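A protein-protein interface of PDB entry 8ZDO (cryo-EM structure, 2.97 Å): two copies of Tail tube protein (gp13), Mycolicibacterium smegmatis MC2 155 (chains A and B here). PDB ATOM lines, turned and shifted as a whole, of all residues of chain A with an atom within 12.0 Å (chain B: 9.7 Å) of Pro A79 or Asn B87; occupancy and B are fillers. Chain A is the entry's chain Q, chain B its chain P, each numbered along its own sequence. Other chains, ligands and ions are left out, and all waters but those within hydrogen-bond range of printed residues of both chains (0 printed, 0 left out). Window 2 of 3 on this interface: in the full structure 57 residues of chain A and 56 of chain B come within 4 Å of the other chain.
OE2 of Glu A78 is in salt-bridge range of NE of Arg B187 (2.6 Å). The guanidinium group of Arg B187 is in salt-bridge range of the side-chain carboxylate of Glu A80 (3.4 Å).
Pro A79 touches just these residues of chain B: Asn B87 (3.3 Å) and Lys B88 (3.4 Å). Of chain A, only Pro A79 comes within 4 Å of Asn B87. Glu A80 touches just one residue of chain B: Arg B187. No residue of chain A comes within 4 Å of Asp B69. No residue of chain A comes within 4 Å of Ser B70. No residue of chain A comes within 4 Å of Lys B71. Ile B85 touches none of the printed residues of chain A. No residue of chain A comes within 4 Å of Ile B86. Lys B88 touches just one residue of chain A: Pro A79 (3.4 Å). Printed residues of chain B within 4 Å of Arg A83: Phe B186 (3.98 Å). Printed residues of chain B within 4 Å of Pro A81: Phe B186. Printed residues of chain A within 4 Å of Arg B187: Glu A78 and Glu A80. Tyr A76 touches none of the printed residues of chain B. The nearest residue of chain A that does not touch Asn B87 is Glu A80 (5.3 Å).
CB of Pro A79 touches O of Asn B87, at 3.3 Å. CE of Lys B88 touches O of Pro A79 (3.4 Å). Pro A81 touches Phe B186. Phe B186 touches Ile A82 (CD2 to O, 3.4 Å). Arg A83 touches Phe B186 (C to CE2, 3.98 Å). Thr A84 touches Phe B186.
Positions printed for both chains: 72, 73 and 84. Of the 8 pairs that touch across the chains among the printed residues, none has its exchanged pair printed and touching as well.
O of Asp B69 is in hydrogen-bond range of N of Asn B87. The side-chain carboxylate (OD2) of Asp B69 is in salt-bridge range of the side-chain amino group (NZ) of Lys B88 (3.5 Å). The side-chain hydroxyl (OG1) of Thr A84 lies close to the side-chain carboxylate (OD1) of Asp A72, 3.3 Å away. The backbone carbonyl oxygen of Ile A73 is in hydrogen-bond range of the backbone NH of Ile A82, at 3.1 Å. O of Arg A83 lies within hydrogen-bond range of N of Ile A73, 2.9 Å away.
Of the 17 printed residues of chain B, 4 touch a printed residue of chain A. Along chain B the printed residues that touch a printed residue of chain A span positions 87 to 187. Hydrophobic or aromatic side chains of chain A that line the printed part of chain B: Pro A79. Among the printed residues, 8 pairs touch across the chains.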
ATOM      1  N   ASP A  72      -8.716 -18.318  14.669  1.00  0.00           N
ATOM      2  CA  ASP A  72      -9.999 -17.736  15.038  1.00  0.00           C
ATOM      3  C   ASP A  72     -11.021 -17.971  13.934  1.00  0.00           C
ATOM      4  O   ASP A  72     -10.725 -17.775  12.753  1.00  0.00           O
ATOM      5  CB  ASP A  72      -9.851 -16.239  15.301  1.00  0.00           C
ATOM      6  CG  ASP A  72      -9.469 -15.931  16.732  1.00  0.00           C
ATOM      7  OD1 ASP A  72      -9.632 -16.816  17.597  1.00  0.00           O
ATOM      8  OD2 ASP A  72      -9.004 -14.802  16.993  1.00  0.00           O
ATOM      9  N   ILE A  73     -12.224 -18.384  14.319  1.00  0.00           N
ATOM     10  CA  ILE A  73     -13.327 -18.585  13.388  1.00  0.00           C
ATOM     11  C   ILE A  73     -14.222 -17.360  13.460  1.00  0.00           C
ATOM     12  O   ILE A  73     -14.696 -16.990  14.541  1.00  0.00           O
ATOM     13  CB  ILE A  73     -14.108 -19.866  13.714  1.00  0.00           C
ATOM     14  CG1 ILE A  73     -13.178 -21.077  13.678  1.00  0.00           C
ATOM     15  CG2 ILE A  73     -15.263 -20.043  12.746  1.00  0.00           C
ATOM     16  CD1 ILE A  73     -12.542 -21.311  12.333  1.00  0.00           C
ATOM     17  N   GLU A  74     -14.452 -16.728  12.316  1.00  0.00           N
ATOM     18  CA  GLU A  74     -15.223 -15.498  12.246  1.00  0.00           C
ATOM     19  C   GLU A  74     -16.605 -15.778  11.676  1.00  0.00           C
ATOM     20  O   GLU A  74     -16.748 -16.530  10.709  1.00  0.00           O
ATOM     21  CB  GLU A  74     -14.505 -14.457  11.388  1.00  0.00           C
ATOM     22  CG  GLU A  74     -13.237 -13.912  12.013  1.00  0.00           C
ATOM     23  CD  GLU A  74     -13.489 -12.676  12.850  1.00  0.00           C
ATOM     24  OE1 GLU A  74     -13.994 -12.816  13.982  1.00  0.00           O
ATOM     25  OE2 GLU A  74     -13.182 -11.562  12.376  1.00  0.00           O
ATOM     26  N   ALA A  75     -17.619 -15.174  12.286  1.00  0.00           N
ATOM     27  CA  ALA A  75     -18.994 -15.308  11.833  1.00  0.00           C
ATOM     28  C   ALA A  75     -19.414 -14.058  11.077  1.00  0.00           C
ATOM     29  O   ALA A  75     -18.974 -12.950  11.394  1.00  0.00           O
ATOM     30  CB  ALA A  75     -19.941 -15.552  13.007  1.00  0.00           C
ATOM     31  N   TYR A  76     -20.265 -14.247  10.069  1.00  0.00           N
ATOM     32  CA  TYR A  76     -20.728 -13.123   9.264  1.00  0.00           C
ATOM     33  C   TYR A  76     -21.557 -12.151  10.092  1.00  0.00           C
ATOM     34  O   TYR A  76     -21.433 -10.931   9.939  1.00  0.00           O
ATOM     35  CB  TYR A  76     -21.529 -13.641   8.074  1.00  0.00           C
ATOM     36  CG  TYR A  76     -22.294 -12.581   7.326  1.00  0.00           C
ATOM     37  CD1 TYR A  76     -21.640 -11.669   6.516  1.00  0.00           C
ATOM     38  CD2 TYR A  76     -23.675 -12.503   7.416  1.00  0.00           C
ATOM     39  CE1 TYR A  76     -22.335 -10.701   5.829  1.00  0.00           C
ATOM     40  CE2 TYR A  76     -24.380 -11.540   6.729  1.00  0.00           C
ATOM     41  CZ  TYR A  76     -23.704 -10.643   5.934  1.00  0.00           C
ATOM     42  OH  TYR A  76     -24.398  -9.677   5.246  1.00  0.00           O
ATOM     43  N   GLY A  77     -22.408 -12.668  10.973  1.00  0.00           N
ATOM     44  CA  GLY A  77     -23.288 -11.824  11.754  1.00  0.00           C
ATOM     45  C   GLY A  77     -22.784 -11.513  13.148  1.00  0.00           C
ATOM     46  O   GLY A  77     -23.567 -11.123  14.019  1.00  0.00           O
ATOM     47  N   GLU A  78     -21.483 -11.683  13.379  1.00  0.00           N
ATOM     48  CA  GLU A  78     -20.896 -11.436  14.687  1.00  0.00           C
ATOM     49  C   GLU A  78     -19.574 -10.699  14.501  1.00  0.00           C
ATOM     50  O   GLU A  78     -18.762 -11.097  13.648  1.00  0.00           O
ATOM     51  CB  GLU A  78     -20.681 -12.746  15.450  1.00  0.00           C
ATOM     52  CG  GLU A  78     -20.615 -12.587  16.958  1.00  0.00           C
ATOM     53  CD  GLU A  78     -21.968 -12.285  17.567  1.00  0.00           C
ATOM     54  OE1 GLU A  78     -22.991 -12.683  16.973  1.00  0.00           O
ATOM     55  OE2 GLU A  78     -22.010 -11.648  18.641  1.00  0.00           O
ATOM     56  N   PRO A  79     -19.325  -9.633  15.264  1.00  0.00           N
ATOM     57  CA  PRO A  79     -18.064  -8.895  15.104  1.00  0.00           C
ATOM     58  C   PRO A  79     -16.859  -9.653  15.641  1.00  0.00           C
ATOM     59  O   PRO A  79     -15.813  -9.705  14.988  1.00  0.00           O
ATOM     60  CB  PRO A  79     -18.313  -7.602  15.888  1.00  0.00           C
ATOM     61  CG  PRO A  79     -19.355  -7.948  16.881  1.00  0.00           C
ATOM     62  CD  PRO A  79     -20.207  -9.025  16.275  1.00  0.00           C
ATOM     63  N   GLU A  80     -16.992 -10.237  16.826  1.00  0.00           N
ATOM     64  CA  GLU A  80     -15.905 -10.979  17.439  1.00  0.00           C
ATOM     65  C   GLU A  80     -15.873 -12.413  16.921  1.00  0.00           C
ATOM     66  O   GLU A  80     -16.861 -12.909  16.375  1.00  0.00           O
ATOM     67  CB  GLU A  80     -16.059 -10.976  18.957  1.00  0.00           C
ATOM     68  CG  GLU A  80     -17.193 -11.857  19.452  1.00  0.00           C
ATOM     69  CD  GLU A  80     -18.506 -11.112  19.552  1.00  0.00           C
ATOM     70  OE1 GLU A  80     -18.568  -9.953  19.098  1.00  0.00           O
ATOM     71  OE2 GLU A  80     -19.483 -11.689  20.067  1.00  0.00           O
ATOM     72  N   PRO A  81     -14.739 -13.097  17.061  1.00  0.00           N
ATOM     73  CA  PRO A  81     -14.693 -14.518  16.696  1.00  0.00           C
ATOM     74  C   PRO A  81     -15.566 -15.350  17.623  1.00  0.00           C
ATOM     75  O   PRO A  81     -15.467 -15.257  18.847  1.00  0.00           O
ATOM     76  CB  PRO A  81     -13.209 -14.876  16.845  1.00  0.00           C
ATOM     77  CG  PRO A  81     -12.490 -13.576  16.756  1.00  0.00           C
ATOM     78  CD  PRO A  81     -13.400 -12.572  17.383  1.00  0.00           C
ATOM     79  N   ILE A  82     -16.432 -16.168  17.024  1.00  0.00           N
ATOM     80  CA  ILE A  82     -17.316 -17.015  17.815  1.00  0.00           C
ATOM     81  C   ILE A  82     -16.532 -18.133  18.494  1.00  0.00           C
ATOM     82  O   ILE A  82     -16.814 -18.495  19.643  1.00  0.00           O
ATOM     83  CB  ILE A  82     -18.462 -17.560  16.943  1.00  0.00           C
ATOM     84  CG1 ILE A  82     -17.921 -18.362  15.759  1.00  0.00           C
ATOM     85  CG2 ILE A  82     -19.343 -16.428  16.462  1.00  0.00           C
ATOM     86  CD1 ILE A  82     -18.989 -19.101  14.986  1.00  0.00           C
ATOM     87  N   ARG A  83     -15.540 -18.695  17.808  1.00  0.00           N
ATOM     88  CA  ARG A  83     -14.758 -19.798  18.341  1.00  0.00           C
ATOM     89  C   ARG A  83     -13.299 -19.626  17.951  1.00  0.00           C
ATOM     90  O   ARG A  83     -12.951 -18.827  17.079  1.00  0.00           O
ATOM     91  CB  ARG A  83     -15.273 -21.152  17.839  1.00  0.00           C
ATOM     92  CG  ARG A  83     -16.545 -21.631  18.511  1.00  0.00           C
ATOM     93  CD  ARG A  83     -17.004 -22.954  17.929  1.00  0.00           C
ATOM     94  NE  ARG A  83     -17.889 -22.775  16.786  1.00  0.00           N
ATOM     95  CZ  ARG A  83     -17.506 -22.875  15.522  1.00  0.00           C
ATOM     96  NH1 ARG A  83     -16.253 -23.145  15.200  1.00  0.00           N
ATOM     97  NH2 ARG A  83     -18.404 -22.700  14.556  1.00  0.00           N
ATOM     98  N   THR A  84     -12.438 -20.387  18.619  1.00  0.00           N
ATOM     99  CA  THR A  84     -11.052 -20.531  18.207  1.00  0.00           C
ATOM    100  C   THR A  84     -10.677 -22.002  18.275  1.00  0.00           C
ATOM    101  O   THR A  84     -11.179 -22.750  19.117  1.00  0.00           O
ATOM    102  CB  THR A  84     -10.101 -19.683  19.065  1.00  0.00           C
ATOM    103  OG1 THR A  84      -8.754 -19.866  18.614  1.00  0.00           O
ATOM    104  CG2 THR A  84     -10.200 -20.063  20.524  1.00  0.00           C
ATOM    105  N   GLU B  67      -8.277  -5.421  24.183  1.00  0.00           N
ATOM    106  CA  GLU B  67      -7.680  -5.122  22.890  1.00  0.00           C
ATOM    107  C   GLU B  67      -8.760  -4.600  21.955  1.00  0.00           C
ATOM    108  O   GLU B  67      -9.784  -5.259  21.756  1.00  0.00           O
ATOM    109  CB  GLU B  67      -7.012  -6.361  22.289  1.00  0.00           C
ATOM    110  CG  GLU B  67      -5.745  -6.791  23.007  1.00  0.00           C
ATOM    111  CD  GLU B  67      -6.014  -7.765  24.139  1.00  0.00           C
ATOM    112  OE1 GLU B  67      -7.158  -8.255  24.246  1.00  0.00           O
ATOM    113  OE2 GLU B  67      -5.082  -8.038  24.924  1.00  0.00           O
ATOM    114  N   PHE B  68      -8.529  -3.421  21.387  1.00  0.00           N
ATOM    115  CA  PHE B  68      -9.488  -2.783  20.497  1.00  0.00           C
ATOM    116  C   PHE B  68      -9.008  -2.906  19.059  1.00  0.00           C
ATOM    117  O   PHE B  68      -7.852  -2.594  18.755  1.00  0.00           O
ATOM    118  CB  PHE B  68      -9.681  -1.303  20.838  1.00  0.00           C
ATOM    119  CG  PHE B  68     -10.405  -1.049  22.134  1.00  0.00           C
ATOM    120  CD1 PHE B  68     -10.598  -2.056  23.062  1.00  0.00           C
ATOM    121  CD2 PHE B  68     -10.911   0.207  22.410  1.00  0.00           C
ATOM    122  CE1 PHE B  68     -11.261  -1.809  24.243  1.00  0.00           C
ATOM    123  CE2 PHE B  68     -11.579   0.456  23.586  1.00  0.00           C
ATOM    124  CZ  PHE B  68     -11.753  -0.553  24.504  1.00  0.00           C
ATOM    125  N   ASP B  69      -9.895  -3.358  18.182  1.00  0.00           N
ATOM    126  CA  ASP B  69      -9.679  -3.289  16.744  1.00  0.00           C
ATOM    127  C   ASP B  69     -10.446  -2.080  16.230  1.00  0.00           C
ATOM    128  O   ASP B  69     -11.669  -2.011  16.379  1.00  0.00           O
ATOM    129  CB  ASP B  69     -10.146  -4.571  16.056  1.00  0.00           C
ATOM    130  CG  ASP B  69      -9.528  -4.757  14.684  1.00  0.00           C
ATOM    131  OD1 ASP B  69      -9.296  -3.748  13.986  1.00  0.00           O
ATOM    132  OD2 ASP B  69      -9.275  -5.918  14.299  1.00  0.00           O
ATOM    133  N   SER B  70      -9.732  -1.123  15.646  1.00  0.00           N
ATOM    134  CA  SER B  70     -10.323   0.143  15.248  1.00  0.00           C
ATOM    135  C   SER B  70     -10.098   0.394  13.764  1.00  0.00           C
ATOM    136  O   SER B  70      -9.175  -0.145  13.149  1.00  0.00           O
ATOM    137  CB  SER B  70      -9.747   1.307  16.065  1.00  0.00           C
ATOM    138  OG  SER B  70     -10.066   1.172  17.438  1.00  0.00           O
ATOM    139  N   LYS B  71     -10.969   1.224  13.196  1.00  0.00           N
ATOM    140  CA  LYS B  71     -10.898   1.588  11.786  1.00  0.00           C
ATOM    141  C   LYS B  71     -11.273   3.054  11.645  1.00  0.00           C
ATOM    142  O   LYS B  71     -12.373   3.452  12.036  1.00  0.00           O
ATOM    143  CB  LYS B  71     -11.830   0.711  10.947  1.00  0.00           C
ATOM    144  CG  LYS B  71     -11.820   1.026   9.467  1.00  0.00           C
ATOM    145  CD  LYS B  71     -12.879   0.226   8.730  1.00  0.00           C
ATOM    146  CE  LYS B  71     -12.782  -1.255   9.055  1.00  0.00           C
ATOM    147  NZ  LYS B  71     -13.840  -2.044   8.367  1.00  0.00           N
ATOM    148  N   ASP B  72     -10.362   3.853  11.097  1.00  0.00           N
ATOM    149  CA  ASP B  72     -10.634   5.266  10.871  1.00  0.00           C
ATOM    150  C   ASP B  72     -11.439   5.452   9.593  1.00  0.00           C
ATOM    151  O   ASP B  72     -11.228   4.750   8.601  1.00  0.00           O
ATOM    152  CB  ASP B  72      -9.331   6.059  10.779  1.00  0.00           C
ATOM    153  CG  ASP B  72      -8.519   5.996  12.053  1.00  0.00           C
ATOM    154  OD1 ASP B  72      -9.026   5.456  13.057  1.00  0.00           O
ATOM    155  OD2 ASP B  72      -7.373   6.492  12.053  1.00  0.00           O
ATOM    156  N   ILE B  73     -12.361   6.409   9.619  1.00  0.00           N
ATOM    157  CA  ILE B  73     -13.179   6.759   8.465  1.00  0.00           C
ATOM    158  C   ILE B  73     -12.683   8.098   7.943  1.00  0.00           C
ATOM    159  O   ILE B  73     -12.654   9.089   8.682  1.00  0.00           O
ATOM    160  CB  ILE B  73     -14.670   6.822   8.827  1.00  0.00           C
ATOM    161  CG1 ILE B  73     -15.141   5.474   9.372  1.00  0.00           C
ATOM    162  CG2 ILE B  73     -15.491   7.225   7.617  1.00  0.00           C
ATOM    163  CD1 ILE B  73     -15.146   4.375   8.343  1.00  0.00           C
ATOM    164  N   THR B  84     -14.159   7.119  14.030  1.00  0.00           N
ATOM    165  CA  THR B  84     -13.499   5.833  14.191  1.00  0.00           C
ATOM    166  C   THR B  84     -14.531   4.803  14.620  1.00  0.00           C
ATOM    167  O   THR B  84     -15.420   5.101  15.420  1.00  0.00           O
ATOM    168  CB  THR B  84     -12.361   5.892  15.218  1.00  0.00           C
ATOM    169  OG1 THR B  84     -12.881   6.284  16.491  1.00  0.00           O
ATOM    170  CG2 THR B  84     -11.296   6.882  14.786  1.00  0.00           C
ATOM    171  N   ILE B  85     -14.414   3.597  14.075  1.00  0.00           N
ATOM    172  CA  ILE B  85     -15.303   2.488  14.396  1.00  0.00           C
ATOM    173  C   ILE B  85     -14.507   1.444  15.158  1.00  0.00           C
ATOM    174  O   ILE B  85     -13.441   1.015  14.703  1.00  0.00           O
ATOM    175  CB  ILE B  85     -15.925   1.877  13.129  1.00  0.00           C
ATOM    176  CG1 ILE B  85     -16.480   2.971  12.221  1.00  0.00           C
ATOM    177  CG2 ILE B  85     -17.015   0.886  13.498  1.00  0.00           C
ATOM    178  CD1 ILE B  85     -17.000   2.449  10.905  1.00  0.00           C
ATOM    179  N   ILE B  86     -15.020   1.042  16.318  1.00  0.00           N
ATOM    180  CA  ILE B  86     -14.442  -0.055  17.086  1.00  0.00           C
ATOM    181  C   ILE B  86     -15.143  -1.328  16.621  1.00  0.00           C
ATOM    182  O   ILE B  86     -16.268  -1.616  17.027  1.00  0.00           O
ATOM    183  CB  ILE B  86     -14.591   0.161  18.591  1.00  0.00           C
ATOM    184  CG1 ILE B  86     -14.070   1.542  18.982  1.00  0.00           C
ATOM    185  CG2 ILE B  86     -13.845  -0.916  19.352  1.00  0.00           C
ATOM    186  CD1 ILE B  86     -14.080   1.793  20.470  1.00  0.00           C
ATOM    187  N   ASN B  87     -14.471  -2.088  15.755  1.00  0.00           N
ATOM    188  CA  ASN B  87     -15.074  -3.295  15.203  1.00  0.00           C
ATOM    189  C   ASN B  87     -15.321  -4.341  16.282  1.00  0.00           C
ATOM    190  O   ASN B  87     -16.382  -4.974  16.306  1.00  0.00           O
ATOM    191  CB  ASN B  87     -14.182  -3.866  14.102  1.00  0.00           C
ATOM    192  CG  ASN B  87     -14.008  -2.909  12.942  1.00  0.00           C
ATOM    193  OD1 ASN B  87     -12.894  -2.484  12.638  1.00  0.00           O
ATOM    194  ND2 ASN B  87     -15.109  -2.566  12.287  1.00  0.00           N
ATOM    195  N   LYS B  88     -14.362  -4.536  17.182  1.00  0.00           N
ATOM    196  CA  LYS B  88     -14.483  -5.564  18.203  1.00  0.00           C
ATOM    197  C   LYS B  88     -13.636  -5.186  19.407  1.00  0.00           C
ATOM    198  O   LYS B  88     -12.765  -4.318  19.334  1.00  0.00           O
ATOM    199  CB  LYS B  88     -14.061  -6.938  17.670  1.00  0.00           C
ATOM    200  CG  LYS B  88     -12.561  -7.105  17.515  1.00  0.00           C
ATOM    201  CD  LYS B  88     -12.197  -8.544  17.210  1.00  0.00           C
ATOM    202  CE  LYS B  88     -12.630  -8.933  15.808  1.00  0.00           C
ATOM    203  NZ  LYS B  88     -11.948  -8.108  14.774  1.00  0.00           N
ATOM    204  N   ARG B  89     -13.908  -5.859  20.522  1.00  0.00           N
ATOM    205  CA  ARG B  89     -13.181  -5.643  21.769  1.00  0.00           C
ATOM    206  C   ARG B  89     -12.893  -7.006  22.378  1.00  0.00           C
ATOM    207  O   ARG B  89     -13.813  -7.686  22.842  1.00  0.00           O
ATOM    208  CB  ARG B  89     -13.984  -4.772  22.733  1.00  0.00           C
ATOM    209  CG  ARG B  89     -13.429  -4.729  24.139  1.00  0.00           C
ATOM    210  CD  ARG B  89     -14.132  -3.671  24.961  1.00  0.00           C
ATOM    211  NE  ARG B  89     -13.543  -3.526  26.285  1.00  0.00           N
ATOM    212  CZ  ARG B  89     -13.733  -2.481  27.075  1.00  0.00           C
ATOM    213  NH1 ARG B  89     -14.491  -1.464  26.704  1.00  0.00           N
ATOM    214  NH2 ARG B  89     -13.145  -2.452  28.268  1.00  0.00           N
ATOM    215  N   THR B  90     -11.625  -7.402  22.379  1.00  0.00           N
ATOM    216  CA  THR B  90     -11.220  -8.702  22.888  1.00  0.00           C
ATOM    217  C   THR B  90     -10.800  -8.574  24.345  1.00  0.00           C
ATOM    218  O   THR B  90     -10.002  -7.702  24.694  1.00  0.00           O
ATOM    219  CB  THR B  90     -10.074  -9.275  22.055  1.00  0.00           C
ATOM    220  OG1 THR B  90     -10.524  -9.508  20.715  1.00  0.00           O
ATOM    221  CG2 THR B  90      -9.577 -10.579  22.650  1.00  0.00           C
ATOM    222  N   LYS B 184      -9.300 -16.366  27.241  1.00  0.00           N
ATOM    223  CA  LYS B 184      -9.972 -15.409  26.378  1.00  0.00           C
ATOM    224  C   LYS B 184     -11.477 -15.552  26.533  1.00  0.00           C
ATOM    225  O   LYS B 184     -12.004 -16.669  26.544  1.00  0.00           O
ATOM    226  CB  LYS B 184      -9.570 -15.629  24.920  1.00  0.00           C
ATOM    227  CG  LYS B 184     -10.003 -14.534  23.970  1.00  0.00           C
ATOM    228  CD  LYS B 184      -9.702 -14.919  22.535  1.00  0.00           C
ATOM    229  CE  LYS B 184     -10.418 -14.010  21.555  1.00  0.00           C
ATOM    230  NZ  LYS B 184     -11.874 -13.914  21.853  1.00  0.00           N
ATOM    231  N   PHE B 186     -15.362 -15.098  25.341  1.00  0.00           N
ATOM    232  CA  PHE B 186     -16.228 -15.071  24.177  1.00  0.00           C
ATOM    233  C   PHE B 186     -17.626 -14.659  24.611  1.00  0.00           C
ATOM    234  O   PHE B 186     -17.987 -14.759  25.785  1.00  0.00           O
ATOM    235  CB  PHE B 186     -16.283 -16.436  23.479  1.00  0.00           C
ATOM    236  CG  PHE B 186     -14.958 -16.909  22.963  1.00  0.00           C
ATOM    237  CD1 PHE B 186     -14.019 -17.454  23.820  1.00  0.00           C
ATOM    238  CD2 PHE B 186     -14.654 -16.817  21.620  1.00  0.00           C
ATOM    239  CE1 PHE B 186     -12.803 -17.888  23.348  1.00  0.00           C
ATOM    240  CE2 PHE B 186     -13.439 -17.251  21.143  1.00  0.00           C
ATOM    241  CZ  PHE B 186     -12.513 -17.787  22.008  1.00  0.00           C
ATOM    242  N   ARG B 187     -18.414 -14.187  23.653  1.00  0.00           N
ATOM    243  CA  ARG B 187     -19.773 -13.765  23.946  1.00  0.00           C
ATOM    244  C   ARG B 187     -20.688 -14.976  24.048  1.00  0.00           C
ATOM    245  O   ARG B 187     -20.744 -15.802  23.133  1.00  0.00           O
ATOM    246  CB  ARG B 187     -20.284 -12.811  22.872  1.00  0.00           C
ATOM    247  CG  ARG B 187     -21.442 -11.940  23.321  1.00  0.00           C
ATOM    248  CD  ARG B 187     -21.961 -11.094  22.181  1.00  0.00           C
ATOM    249  NE  ARG B 187     -22.657 -11.893  21.183  1.00  0.00           N
ATOM    250  CZ  ARG B 187     -23.948 -12.189  21.226  1.00  0.00           C
ATOM    251  NH1 ARG B 187     -24.722 -11.759  22.210  1.00  0.00           N
ATOM    252  NH2 ARG B 187     -24.478 -12.933  20.260  1.00  0.00           N
